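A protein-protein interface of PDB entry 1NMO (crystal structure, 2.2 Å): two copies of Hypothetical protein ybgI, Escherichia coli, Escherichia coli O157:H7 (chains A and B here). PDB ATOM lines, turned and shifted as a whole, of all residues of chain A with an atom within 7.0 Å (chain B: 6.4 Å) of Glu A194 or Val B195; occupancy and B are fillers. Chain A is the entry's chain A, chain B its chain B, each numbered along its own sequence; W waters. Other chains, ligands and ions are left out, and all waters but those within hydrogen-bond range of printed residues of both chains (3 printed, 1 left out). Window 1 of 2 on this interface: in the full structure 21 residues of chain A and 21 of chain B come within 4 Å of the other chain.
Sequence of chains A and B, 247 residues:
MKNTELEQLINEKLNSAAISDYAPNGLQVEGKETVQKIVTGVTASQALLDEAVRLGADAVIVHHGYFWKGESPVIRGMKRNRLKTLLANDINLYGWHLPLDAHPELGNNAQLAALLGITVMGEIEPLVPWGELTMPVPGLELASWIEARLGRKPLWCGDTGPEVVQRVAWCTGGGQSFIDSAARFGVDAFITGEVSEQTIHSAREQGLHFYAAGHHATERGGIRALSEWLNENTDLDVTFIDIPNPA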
ATOM      1  N   ARG A 152     -14.873   1.422   2.053  1.00  0.00           N
ATOM      2  CA  ARG A 152     -15.148   2.756   2.615  1.00  0.00           C
ATOM      3  C   ARG A 152     -13.969   3.208   3.430  1.00  0.00           C
ATOM      4  O   ARG A 152     -13.459   2.444   4.206  1.00  0.00           O
ATOM      5  CB  ARG A 152     -16.396   2.698   3.560  1.00  0.00           C
ATOM      6  CG  ARG A 152     -16.702   4.041   4.368  1.00  0.00           C
ATOM      7  CD  ARG A 152     -17.928   3.894   5.259  1.00  0.00           C
ATOM      8  NE  ARG A 152     -18.421   5.147   5.826  1.00  0.00           N
ATOM      9  CZ  ARG A 152     -17.994   5.686   6.968  1.00  0.00           C
ATOM     10  NH1 ARG A 152     -17.060   5.077   7.671  1.00  0.00           N
ATOM     11  NH2 ARG A 152     -18.518   6.847   7.410  1.00  0.00           N
ATOM     12  N   CYS A 171     -16.908  -3.024  18.155  1.00  0.00           N
ATOM     13  CA  CYS A 171     -18.359  -3.167  18.344  1.00  0.00           C
ATOM     14  C   CYS A 171     -18.883  -2.575  17.059  1.00  0.00           C
ATOM     15  O   CYS A 171     -18.555  -1.450  16.804  1.00  0.00           O
ATOM     16  CB  CYS A 171     -18.911  -2.355  19.537  1.00  0.00           C
ATOM     17  SG  CYS A 171     -20.734  -2.604  19.691  1.00  0.00           S
ATOM     18  N   THR A 172     -19.652  -3.297  16.238  1.00  0.00           N
ATOM     19  CA  THR A 172     -20.120  -2.685  15.025  1.00  0.00           C
ATOM     20  C   THR A 172     -21.235  -1.578  15.294  1.00  0.00           C
ATOM     21  O   THR A 172     -21.840  -1.524  16.343  1.00  0.00           O
ATOM     22  CB  THR A 172     -20.753  -3.723  14.079  1.00  0.00           C
ATOM     23  OG1 THR A 172     -21.967  -4.183  14.696  1.00  0.00           O
ATOM     24  CG2 THR A 172     -19.768  -4.884  13.710  1.00  0.00           C
ATOM     25  N   GLY A 173     -21.463  -0.667  14.351  1.00  0.00           N
ATOM     26  CA  GLY A 173     -22.529   0.294  14.557  1.00  0.00           C
ATOM     27  C   GLY A 173     -22.187   1.464  15.411  1.00  0.00           C
ATOM     28  O   GLY A 173     -21.078   2.006  15.312  1.00  0.00           O
ATOM     29  N   GLY A 174     -23.127   1.895  16.241  1.00  0.00           N
ATOM     30  CA  GLY A 174     -22.811   3.026  17.107  1.00  0.00           C
ATOM     31  C   GLY A 174     -22.202   2.553  18.424  1.00  0.00           C
ATOM     32  O   GLY A 174     -22.804   2.795  19.480  1.00  0.00           O
ATOM     33  N   GLY A 175     -21.056   1.844  18.369  1.00  0.00           N
ATOM     34  CA  GLY A 175     -20.420   1.359  19.580  1.00  0.00           C
ATOM     35  C   GLY A 175     -19.316   2.245  20.134  1.00  0.00           C
ATOM     36  O   GLY A 175     -18.583   1.825  21.006  1.00  0.00           O
ATOM     37  N   GLN A 176     -19.208   3.491  19.670  1.00  0.00           N
ATOM     38  CA  GLN A 176     -18.128   4.363  20.112  1.00  0.00           C
ATOM     39  C   GLN A 176     -18.034   4.518  21.594  1.00  0.00           C
ATOM     40  O   GLN A 176     -16.982   4.864  22.113  1.00  0.00           O
ATOM     41  CB  GLN A 176     -18.298   5.844  19.694  1.00  0.00           C
ATOM     42  CG  GLN A 176     -18.994   6.276  18.442  1.00  0.00           C
ATOM     43  CD  GLN A 176     -20.511   6.174  18.442  1.00  0.00           C
ATOM     44  OE1 GLN A 176     -21.026   5.066  18.314  1.00  0.00           O
ATOM     45  NE2 GLN A 176     -21.243   7.335  18.533  1.00  0.00           N
ATOM     46  N   SER A 177     -19.162   4.397  22.295  1.00  0.00           N
ATOM     47  CA  SER A 177     -19.074   4.701  23.720  1.00  0.00           C
ATOM     48  C   SER A 177     -18.372   3.594  24.499  1.00  0.00           C
ATOM     49  O   SER A 177     -18.092   3.744  25.709  1.00  0.00           O
ATOM     50  CB  SER A 177     -20.486   5.019  24.275  1.00  0.00           C
ATOM     51  OG  SER A 177     -21.282   3.858  24.287  1.00  0.00           O
ATOM     52  N   PHE A 190      -9.309   0.017  18.701  1.00  0.00           N
ATOM     53  CA  PHE A 190     -10.780  -0.192  18.933  1.00  0.00           C
ATOM     54  C   PHE A 190     -11.402   0.253  17.653  1.00  0.00           C
ATOM     55  O   PHE A 190     -11.055   1.330  17.135  1.00  0.00           O
ATOM     56  CB  PHE A 190     -11.339   0.651  20.104  1.00  0.00           C
ATOM     57  CG  PHE A 190     -12.823   0.512  20.286  1.00  0.00           C
ATOM     58  CD1 PHE A 190     -13.397  -0.707  20.636  1.00  0.00           C
ATOM     59  CD2 PHE A 190     -13.681   1.625  20.108  1.00  0.00           C
ATOM     60  CE1 PHE A 190     -14.806  -0.853  20.825  1.00  0.00           C
ATOM     61  CE2 PHE A 190     -15.056   1.506  20.290  1.00  0.00           C
ATOM     62  CZ  PHE A 190     -15.641   0.242  20.656  1.00  0.00           C
ATOM     63  N   ILE A 191     -12.306  -0.564  17.113  1.00  0.00           N
ATOM     64  CA  ILE A 191     -12.971  -0.303  15.837  1.00  0.00           C
ATOM     65  C   ILE A 191     -14.466  -0.260  16.016  1.00  0.00           C
ATOM     66  O   ILE A 191     -15.019  -1.181  16.644  1.00  0.00           O
ATOM     67  CB  ILE A 191     -12.732  -1.479  14.835  1.00  0.00           C
ATOM     68  CG1 ILE A 191     -11.268  -1.743  14.722  1.00  0.00           C
ATOM     69  CG2 ILE A 191     -13.314  -1.153  13.395  1.00  0.00           C
ATOM     70  CD1 ILE A 191     -10.989  -2.951  13.906  1.00  0.00           C
ATOM     71  N   THR A 192     -15.181   0.754  15.527  1.00  0.00           N
ATOM     72  CA  THR A 192     -16.633   0.607  15.721  1.00  0.00           C
ATOM     73  C   THR A 192     -17.223   1.238  14.493  1.00  0.00           C
ATOM     74  O   THR A 192     -16.524   1.336  13.501  1.00  0.00           O
ATOM     75  CB  THR A 192     -17.088   1.263  16.985  1.00  0.00           C
ATOM     76  OG1 THR A 192     -18.507   1.078  17.104  1.00  0.00           O
ATOM     77  CG2 THR A 192     -16.800   2.773  16.955  1.00  0.00           C
ATOM     78  N   GLY A 193     -18.474   1.682  14.501  1.00  0.00           N
ATOM     79  CA  GLY A 193     -18.974   2.275  13.249  1.00  0.00           C
ATOM     80  C   GLY A 193     -18.976   3.806  13.222  1.00  0.00           C
ATOM     81  O   GLY A 193     -18.513   4.448  12.298  1.00  0.00           O
ATOM     82  N   GLU A 194     -19.511   4.397  14.272  1.00  0.00           N
ATOM     83  CA  GLU A 194     -19.624   5.843  14.348  1.00  0.00           C
ATOM     84  C   GLU A 194     -18.600   6.426  15.310  1.00  0.00           C
ATOM     85  O   GLU A 194     -17.865   5.689  15.989  1.00  0.00           O
ATOM     86  CB  GLU A 194     -21.020   6.201  14.831  1.00  0.00           C
ATOM     87  CG  GLU A 194     -22.108   5.428  14.229  1.00  0.00           C
ATOM     88  CD  GLU A 194     -23.438   6.139  14.441  1.00  0.00           C
ATOM     89  OE1 GLU A 194     -23.393   7.144  15.194  1.00  0.00           O
ATOM     90  OE2 GLU A 194     -24.519   5.720  13.872  1.00  0.00           O
ATOM     91  N   VAL A 195     -18.568   7.762  15.362  1.00  0.00           N
ATOM     92  CA  VAL A 195     -17.659   8.493  16.217  1.00  0.00           C
ATOM     93  C   VAL A 195     -18.394   9.709  16.823  1.00  0.00           C
ATOM     94  O   VAL A 195     -19.271  10.312  16.169  1.00  0.00           O
ATOM     95  CB  VAL A 195     -16.396   8.962  15.419  1.00  0.00           C
ATOM     96  CG1 VAL A 195     -16.758  10.084  14.434  1.00  0.00           C
ATOM     97  CG2 VAL A 195     -15.278   9.445  16.359  1.00  0.00           C
ATOM     98  N   SER A 196     -18.088  10.031  18.089  1.00  0.00           N
ATOM     99  CA  SER A 196     -18.648  11.235  18.669  1.00  0.00           C
ATOM    100  C   SER A 196     -17.498  12.159  19.097  1.00  0.00           C
ATOM    101  O   SER A 196     -16.262  11.820  19.020  1.00  0.00           O
ATOM    102  CB  SER A 196     -19.567  10.938  19.846  1.00  0.00           C
ATOM    103  OG  SER A 196     -20.694  10.211  19.366  1.00  0.00           O
ATOM    104  N   THR A 199     -15.149  10.587  21.829  1.00  0.00           N
ATOM    105  CA  THR A 199     -14.411   9.404  21.380  1.00  0.00           C
ATOM    106  C   THR A 199     -12.947   9.746  21.045  1.00  0.00           C
ATOM    107  O   THR A 199     -12.002   8.996  21.380  1.00  0.00           O
ATOM    108  CB  THR A 199     -15.019   8.825  20.073  1.00  0.00           C
ATOM    109  OG1 THR A 199     -16.466   8.830  20.114  1.00  0.00           O
ATOM    110  CG2 THR A 199     -14.516   7.388  19.875  1.00  0.00           C
ATOM    111  N   PHE A 210      -7.907   4.404  16.942  1.00  0.00           N
ATOM    112  CA  PHE A 210      -9.364   4.317  16.884  1.00  0.00           C
ATOM    113  C   PHE A 210      -9.797   4.447  15.422  1.00  0.00           C
ATOM    114  O   PHE A 210      -9.227   5.264  14.719  1.00  0.00           O
ATOM    115  CB  PHE A 210     -10.051   5.422  17.730  1.00  0.00           C
ATOM    116  CG  PHE A 210     -11.468   5.565  17.406  1.00  0.00           C
ATOM    117  CD1 PHE A 210     -12.376   4.582  17.779  1.00  0.00           C
ATOM    118  CD2 PHE A 210     -11.908   6.622  16.622  1.00  0.00           C
ATOM    119  CE1 PHE A 210     -13.724   4.627  17.388  1.00  0.00           C
ATOM    120  CE2 PHE A 210     -13.258   6.678  16.219  1.00  0.00           C
ATOM    121  CZ  PHE A 210     -14.158   5.668  16.610  1.00  0.00           C
ATOM    122  N   TYR A 211     -10.772   3.655  14.992  1.00  0.00           N
ATOM    123  CA  TYR A 211     -11.295   3.643  13.617  1.00  0.00           C
ATOM    124  C   TYR A 211     -12.818   3.743  13.715  1.00  0.00           C
ATOM    125  O   TYR A 211     -13.423   2.981  14.495  1.00  0.00           O
ATOM    126  CB  TYR A 211     -11.016   2.300  12.897  1.00  0.00           C
ATOM    127  CG  TYR A 211      -9.564   2.003  12.830  1.00  0.00           C
ATOM    128  CD1 TYR A 211      -8.892   1.534  13.922  1.00  0.00           C
ATOM    129  CD2 TYR A 211      -8.838   2.371  11.699  1.00  0.00           C
ATOM    130  CE1 TYR A 211      -7.484   1.466  13.904  1.00  0.00           C
ATOM    131  CE2 TYR A 211      -7.475   2.293  11.645  1.00  0.00           C
ATOM    132  CZ  TYR A 211      -6.781   1.847  12.754  1.00  0.00           C
ATOM    133  OH  TYR A 211      -5.367   1.820  12.677  1.00  0.00           O
ATOM    134  N   ALA A 212     -13.436   4.662  12.938  1.00  0.00           N
ATOM    135  CA  ALA A 212     -14.907   4.781  12.943  1.00  0.00           C
ATOM    136  C   ALA A 212     -15.075   4.274  11.538  1.00  0.00           C
ATOM    137  O   ALA A 212     -14.847   5.027  10.598  1.00  0.00           O
ATOM    138  CB  ALA A 212     -15.322   6.219  13.059  1.00  0.00           C
ATOM    139  N   ALA A 213     -15.435   2.995  11.366  1.00  0.00           N
ATOM    140  CA  ALA A 213     -15.439   2.419  10.025  1.00  0.00           C
ATOM    141  C   ALA A 213     -16.716   2.519   9.281  1.00  0.00           C
ATOM    142  O   ALA A 213     -16.818   1.949   8.184  1.00  0.00           O
ATOM    143  CB  ALA A 213     -14.994   0.992  10.075  1.00  0.00           C
ATOM    144  N   GLY A 214     -17.686   3.242   9.863  1.00  0.00           N
ATOM    145  CA  GLY A 214     -18.982   3.405   9.221  1.00  0.00           C
ATOM    146  C   GLY A 214     -20.075   2.583   9.863  1.00  0.00           C
ATOM    147  O   GLY A 214     -19.885   1.407  10.110  1.00  0.00           O
ATOM    148  N   HIS A 215     -21.249   3.157  10.106  1.00  0.00           N
ATOM    149  CA  HIS A 215     -22.317   2.374  10.730  1.00  0.00           C
ATOM    150  C   HIS A 215     -22.879   1.311   9.802  1.00  0.00           C
ATOM    151  O   HIS A 215     -22.934   0.078  10.122  1.00  0.00           O
ATOM    152  CB  HIS A 215     -23.475   3.253  11.182  1.00  0.00           C
ATOM    153  CG  HIS A 215     -24.411   2.534  12.093  1.00  0.00           C
ATOM    154  ND1 HIS A 215     -24.840   3.054  13.303  1.00  0.00           N
ATOM    155  CD2 HIS A 215     -25.058   1.359  11.943  1.00  0.00           C
ATOM    156  CE1 HIS A 215     -25.730   2.240  13.849  1.00  0.00           C
ATOM    157  NE2 HIS A 215     -25.875   1.199  13.041  1.00  0.00           N
ATOM    158  N   HIS A 216     -23.402   1.791   8.681  1.00  0.00           N
ATOM    159  CA  HIS A 216     -23.901   0.847   7.658  1.00  0.00           C
ATOM    160  C   HIS A 216     -22.794  -0.126   7.138  1.00  0.00           C
ATOM    161  O   HIS A 216     -23.038  -1.351   6.966  1.00  0.00           O
ATOM    162  CB  HIS A 216     -24.408   1.608   6.465  1.00  0.00           C
ATOM    163  CG  HIS A 216     -24.829   0.719   5.348  1.00  0.00           C
ATOM    164  ND1 HIS A 216     -26.142   0.286   5.188  1.00  0.00           N
ATOM    165  CD2 HIS A 216     -24.124   0.214   4.304  1.00  0.00           C
ATOM    166  CE1 HIS A 216     -26.222  -0.445   4.085  1.00  0.00           C
ATOM    167  NE2 HIS A 216     -25.015  -0.502   3.529  1.00  0.00           N
ATOM    168  N   THR A 218     -20.250  -1.398   8.583  1.00  0.00           N
ATOM    169  CA  THR A 218     -19.954  -2.472   9.498  1.00  0.00           C
ATOM    170  C   THR A 218     -21.104  -3.410   9.877  1.00  0.00           C
ATOM    171  O   THR A 218     -20.860  -4.466  10.551  1.00  0.00           O
ATOM    172  CB  THR A 218     -19.292  -1.915  10.790  1.00  0.00           C
ATOM    173  OG1 THR A 218     -20.209  -1.012  11.464  1.00  0.00           O
ATOM    174  CG2 THR A 218     -17.960  -1.119  10.402  1.00  0.00           C
ATOM    175  N   ASN A 245     -25.312   3.569   2.430  1.00  0.00           N
ATOM    176  CA  ASN A 245     -25.624   4.620   3.385  1.00  0.00           C
ATOM    177  C   ASN A 245     -24.187   5.064   3.805  1.00  0.00           C
ATOM    178  O   ASN A 245     -23.349   4.201   4.161  1.00  0.00           O
ATOM    179  CB  ASN A 245     -26.434   3.999   4.536  1.00  0.00           C
ATOM    180  CG  ASN A 245     -26.767   5.017   5.656  1.00  0.00           C
ATOM    181  OD1 ASN A 245     -26.011   6.007   5.866  1.00  0.00           O
ATOM    182  ND2 ASN A 245     -27.868   4.765   6.404  1.00  0.00           N
ATOM    183  N   PRO A 246     -23.837   6.386   3.724  1.00  0.00           N
ATOM    184  CA  PRO A 246     -22.442   6.744   4.122  1.00  0.00           C
ATOM    185  C   PRO A 246     -22.135   6.811   5.586  1.00  0.00           C
ATOM    186  O   PRO A 246     -20.931   6.753   6.001  1.00  0.00           O
ATOM    187  CB  PRO A 246     -22.204   8.109   3.473  1.00  0.00           C
ATOM    188  CG  PRO A 246     -23.621   8.696   3.413  1.00  0.00           C
ATOM    189  CD  PRO A 246     -24.442   7.442   2.922  1.00  0.00           C
ATOM    190  N   ALA A 247     -23.191   6.860   6.393  1.00  0.00           N
ATOM    191  CA  ALA A 247     -23.017   6.992   7.818  1.00  0.00           C
ATOM    192  C   ALA A 247     -22.583   5.680   8.512  1.00  0.00           C
ATOM    193  O   ALA A 247     -21.967   5.801   9.600  1.00  0.00           O
ATOM    194  CB  ALA A 247     -24.352   7.541   8.450  1.00  0.00           C
ATOM    195  OXT ALA A 247     -22.880   4.566   7.963  1.00  0.00           O
ATOM    196  N   LEU B 155     -20.192  16.064   5.548  1.00  0.00           N
ATOM    197  CA  LEU B 155     -20.829  14.947   4.862  1.00  0.00           C
ATOM    198  C   LEU B 155     -22.104  15.666   4.342  1.00  0.00           C
ATOM    199  O   LEU B 155     -22.783  16.363   5.120  1.00  0.00           O
ATOM    200  CB  LEU B 155     -21.244  13.910   5.881  1.00  0.00           C
ATOM    201  CG  LEU B 155     -22.171  12.826   5.324  1.00  0.00           C
ATOM    202  CD1 LEU B 155     -21.409  12.048   4.284  1.00  0.00           C
ATOM    203  CD2 LEU B 155     -22.522  11.853   6.458  1.00  0.00           C
ATOM    204  N   GLY B 173     -23.471  20.424  17.109  1.00  0.00           N
ATOM    205  CA  GLY B 173     -23.162  19.199  17.870  1.00  0.00           C
ATOM    206  C   GLY B 173     -23.835  17.944  17.417  1.00  0.00           C
ATOM    207  O   GLY B 173     -24.021  17.708  16.231  1.00  0.00           O
ATOM    208  N   GLN B 176     -28.454  15.390  15.242  1.00  0.00           N
ATOM    209  CA  GLN B 176     -29.098  14.665  14.127  1.00  0.00           C
ATOM    210  C   GLN B 176     -30.508  14.148  14.399  1.00  0.00           C
ATOM    211  O   GLN B 176     -31.240  13.864  13.442  1.00  0.00           O
ATOM    212  CB  GLN B 176     -28.351  13.398  13.721  1.00  0.00           C
ATOM    213  CG  GLN B 176     -26.863  13.327  13.917  1.00  0.00           C
ATOM    214  CD  GLN B 176     -26.381  13.056  15.347  1.00  0.00           C
ATOM    215  OE1 GLN B 176     -25.976  14.001  16.029  1.00  0.00           O
ATOM    216  NE2 GLN B 176     -26.355  11.796  15.775  1.00  0.00           N
ATOM    217  N   THR B 192     -26.265  19.994  11.010  1.00  0.00           N
ATOM    218  CA  THR B 192     -25.884  19.661  12.375  1.00  0.00           C
ATOM    219  C   THR B 192     -24.400  19.260  12.457  1.00  0.00           C
ATOM    220  O   THR B 192     -23.663  19.365  11.467  1.00  0.00           O
ATOM    221  CB  THR B 192     -26.796  18.549  12.940  1.00  0.00           C
ATOM    222  OG1 THR B 192     -26.648  18.528  14.363  1.00  0.00           O
ATOM    223  CG2 THR B 192     -26.378  17.109  12.363  1.00  0.00           C
ATOM    224  N   GLY B 193     -23.920  18.829  13.623  1.00  0.00           N
ATOM    225  CA  GLY B 193     -22.510  18.454  13.679  1.00  0.00           C
ATOM    226  C   GLY B 193     -22.274  16.986  13.407  1.00  0.00           C
ATOM    227  O   GLY B 193     -21.437  16.657  12.563  1.00  0.00           O
ATOM    228  N   GLU B 194     -22.993  16.070  14.062  1.00  0.00           N
ATOM    229  CA  GLU B 194     -22.664  14.644  13.815  1.00  0.00           C
ATOM    230  C   GLU B 194     -23.707  13.998  12.932  1.00  0.00           C
ATOM    231  O   GLU B 194     -24.735  14.647  12.603  1.00  0.00           O
ATOM    232  CB  GLU B 194     -22.614  13.827  15.112  1.00  0.00           C
ATOM    233  CG  GLU B 194     -21.814  14.451  16.221  1.00  0.00           C
ATOM    234  CD  GLU B 194     -21.478  13.470  17.389  1.00  0.00           C
ATOM    235  OE1 GLU B 194     -22.149  12.403  17.515  1.00  0.00           O
ATOM    236  OE2 GLU B 194     -20.546  13.788  18.204  1.00  0.00           O
ATOM    237  N   VAL B 195     -23.476  12.717  12.590  1.00  0.00           N
ATOM    238  CA  VAL B 195     -24.443  11.921  11.802  1.00  0.00           C
ATOM    239  C   VAL B 195     -24.685  10.537  12.416  1.00  0.00           C
ATOM    240  O   VAL B 195     -23.914  10.075  13.268  1.00  0.00           O
ATOM    241  CB  VAL B 195     -24.003  11.741  10.310  1.00  0.00           C
ATOM    242  CG1 VAL B 195     -22.948  10.684  10.199  1.00  0.00           C
ATOM    243  CG2 VAL B 195     -25.189  11.282   9.486  1.00  0.00           C
ATOM    244  N   SER B 196     -25.804   9.896  12.063  1.00  0.00           N
ATOM    245  CA  SER B 196     -26.112   8.542  12.553  1.00  0.00           C
ATOM    246  C   SER B 196     -26.648   7.743  11.373  1.00  0.00           C
ATOM    247  O   SER B 196     -27.055   8.313  10.335  1.00  0.00           O
ATOM    248  CB  SER B 196     -27.207   8.530  13.640  1.00  0.00           C
ATOM    249  OG  SER B 196     -26.694   8.997  14.863  1.00  0.00           O
ATOM    250  N   GLU B 197     -26.703   6.441  11.522  1.00  0.00           N
ATOM    251  CA  GLU B 197     -27.226   5.626  10.415  1.00  0.00           C
ATOM    252  C   GLU B 197     -28.618   6.051   9.972  1.00  0.00           C
ATOM    253  O   GLU B 197     -28.827   6.137   8.803  1.00  0.00           O
ATOM    254  CB  GLU B 197     -27.297   4.147  10.803  1.00  0.00           C
ATOM    255  CG  GLU B 197     -27.562   3.145   9.614  1.00  0.00           C
ATOM    256  CD  GLU B 197     -28.997   2.860   9.397  1.00  0.00           C
ATOM    257  OE1 GLU B 197     -29.804   3.252  10.276  1.00  0.00           O
ATOM    258  OE2 GLU B 197     -29.333   2.247   8.350  1.00  0.00           O
ATOM    259  N   GLN B 198     -29.574   6.337  10.870  1.00  0.00           N
ATOM    260  CA  GLN B 198     -30.939   6.676  10.425  1.00  0.00           C
ATOM    261  C   GLN B 198     -31.079   8.103   9.872  1.00  0.00           C
ATOM    262  O   GLN B 198     -32.038   8.490   9.181  1.00  0.00           O
ATOM    263  CB  GLN B 198     -31.890   6.498  11.603  1.00  0.00           C
ATOM    264  CG  GLN B 198     -31.474   7.352  12.822  1.00  0.00           C
ATOM    265  CD  GLN B 198     -30.768   6.535  13.928  1.00  0.00           C
ATOM    266  OE1 GLN B 198     -29.820   5.747  13.654  1.00  0.00           O
ATOM    267  NE2 GLN B 198     -31.215   6.710  15.195  1.00  0.00           N
ATOM    268  N   THR B 199     -30.142   8.936  10.234  1.00  0.00           N
ATOM    269  CA  THR B 199     -30.228  10.321   9.788  1.00  0.00           C
ATOM    270  C   THR B 199     -30.275  10.373   8.265  1.00  0.00           C
ATOM    271  O   THR B 199     -30.926  11.241   7.676  1.00  0.00           O
ATOM    272  CB  THR B 199     -29.014  11.086  10.258  1.00  0.00           C
ATOM    273  OG1 THR B 199     -28.834  10.862  11.651  1.00  0.00           O
ATOM    274  CG2 THR B 199     -29.184  12.527  10.049  1.00  0.00           C
ATOM    275  N   ILE B 200     -29.562   9.464   7.604  1.00  0.00           N
ATOM    276  CA  ILE B 200     -29.496   9.476   6.140  1.00  0.00           C
ATOM    277  C   ILE B 200     -30.842   9.143   5.513  1.00  0.00           C
ATOM    278  O   ILE B 200     -31.182   9.742   4.519  1.00  0.00           O
ATOM    279  CB  ILE B 200     -28.398   8.470   5.659  1.00  0.00           C
ATOM    280  CG1 ILE B 200     -27.036   8.964   6.124  1.00  0.00           C
ATOM    281  CG2 ILE B 200     -28.472   8.255   4.142  1.00  0.00           C
ATOM    282  CD1 ILE B 200     -26.796  10.408   5.607  1.00  0.00           C
ATOM    283  N   PHE B 210     -29.105  17.199   3.782  1.00  0.00           N
ATOM    284  CA  PHE B 210     -28.542  17.060   5.124  1.00  0.00           C
ATOM    285  C   PHE B 210     -27.034  17.336   5.108  1.00  0.00           C
ATOM    286  O   PHE B 210     -26.352  16.953   4.183  1.00  0.00           O
ATOM    287  CB  PHE B 210     -28.749  15.664   5.680  1.00  0.00           C
ATOM    288  CG  PHE B 210     -28.005  15.426   6.986  1.00  0.00           C
ATOM    289  CD1 PHE B 210     -28.364  16.114   8.155  1.00  0.00           C
ATOM    290  CD2 PHE B 210     -26.967  14.493   7.024  1.00  0.00           C
ATOM    291  CE1 PHE B 210     -27.670  15.851   9.396  1.00  0.00           C
ATOM    292  CE2 PHE B 210     -26.233  14.197   8.246  1.00  0.00           C
ATOM    293  CZ  PHE B 210     -26.586  14.871   9.423  1.00  0.00           C
ATOM    294  N   ALA B 212     -23.587  17.132   7.792  1.00  0.00           N
ATOM    295  CA  ALA B 212     -23.121  16.849   9.172  1.00  0.00           C
ATOM    296  C   ALA B 212     -21.817  17.618   9.044  1.00  0.00           C
ATOM    297  O   ALA B 212     -20.934  17.212   8.257  1.00  0.00           O
ATOM    298  CB  ALA B 212     -22.847  15.357   9.386  1.00  0.00           C
HETATM  299  O   HOH W   1     -20.387  12.060  13.778  1.00  0.00           O
HETATM  300  O   HOH W   2     -28.410   1.866   5.999  1.00  0.00           O
HETATM  301  O   HOH W   3     -20.631   9.075  12.879  1.00  0.00           O
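Glu A194 touches Val B195, and with the chains exchanged Val A195 touches Glu B194.
Glu A194 touches Ser B196, and with the chains exchanged Ser A196 touches Glu B194.
Positions printed for both chains: 173, 176, 192, 193, 194, 195, 196, 199, 210 and 212.
Of the 12 pairs that touch across the chains among the printed residues, 4 have their exchanged pair printed and touching as well.
Water W2 lies within hydrogen-bond range of OE2 of Glu B197 (2.6 Å), ND1 of His A216 (2.9 Å) and ND2 of Asn A245 (3.0 Å).
Water W1 bridges the backbone carbonyl oxygen (O) of Val A195 (3.2 Å) and the backbone NH (N) of Val B195 (3.4 Å).
Water W3 lies within hydrogen-bond range of O of Val B195 (3.5 Å) and N of Val A195 (3.5 Å).
The side-chain carboxylate of Glu A194 sits at hydrogen-bond distance from a ring nitrogen (ND1) of His A215, at 2.7 Å.
The backbone NH (N) of Ser A196 is in hydrogen-bond range of the side-chain hydroxyl (OG1) of Thr A199, at 2.9 Å.
N of His A215 lies within hydrogen-bond range of O of Ala A247 (2.8 Å).
The backbone NH (N) of Glu B194 sits at hydrogen-bond distance from the backbone carbonyl oxygen (O) of Gly B173 (2.9 Å).
The backbone NH (N) of Ser B196 is in hydrogen-bond range of the side-chain hydroxyl (OG1) of Thr B199 (3.2 Å).
Hydrophobic or aromatic side chains of chain A that line the printed part of chain B: His A215 and Ala A247.
Of the 14 printed residues of chain B, 5 touch a printed residue of chain A.
Hydrophobic or aromatic side chains of chain B within 4 Å of the printed part of chain A: Val B195 and Ile B200.
Along chain B the printed residues that touch a printed residue of chain A span positions 194 to 200.
Among the printed residues, 12 pairs touch across the chains.
Among the printed residues, no Asp or Glu carboxylate lies within 4 Å of a Lys or Arg side-chain nitrogen of the other chain.
Ser A177 touches none of the printed residues of chain B.
Phe A190 touches none of the printed residues of chain B.
Glu A194 touches three residues of chain B.
Of the printed residues of chain B, His A215 touches Glu B197.
Of chain A, only Glu A194 and Ala A247 come within 4 Å of Val B195.
Printed residues of chain A within 4 Å of Ser B196: Glu A194 and Ala A247.
The nearest residue of chain A that does not touch Val B195 is Val A195 (5.5 Å).
The nearest printed residue of chain A that does not touch Ser B196 is Asn A245 (5.1 Å).
OE2 of Glu A194 lies within hydrogen-bond range of N of Glu B197, at 3.3 Å.
The side-chain carboxylate (OE1) of Glu B194 is in hydrogen-bond range of the side-chain hydroxyl (OG) of Ser A196 (3.2 Å).
The backbone carbonyl oxygen (O) of Glu B197 sits at hydrogen-bond distance from the side-chain amide nitrogen (ND2) of Asn A245, at 2.9 Å.
OE1 of Glu A194 touches O of Val B195, 3.5 Å away.
CA of Ser B196 touches OE2 of Glu A194, 3.5 Å away.
Val A195 touches Glu B194.
His A215 touches Glu B197 (CG to CB, 3.5 Å).
Asn A245 touches Ile B200.
Ala A247 touches Val B195.
Ala A247 touches Ser B196 (CB to O, 3.4 Å).
Glu B197 touches Ala A247 (CA to CB, 3.97 Å).
Ile B200 touches Ala A247 (CG1 to CB, 3.8 Å).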
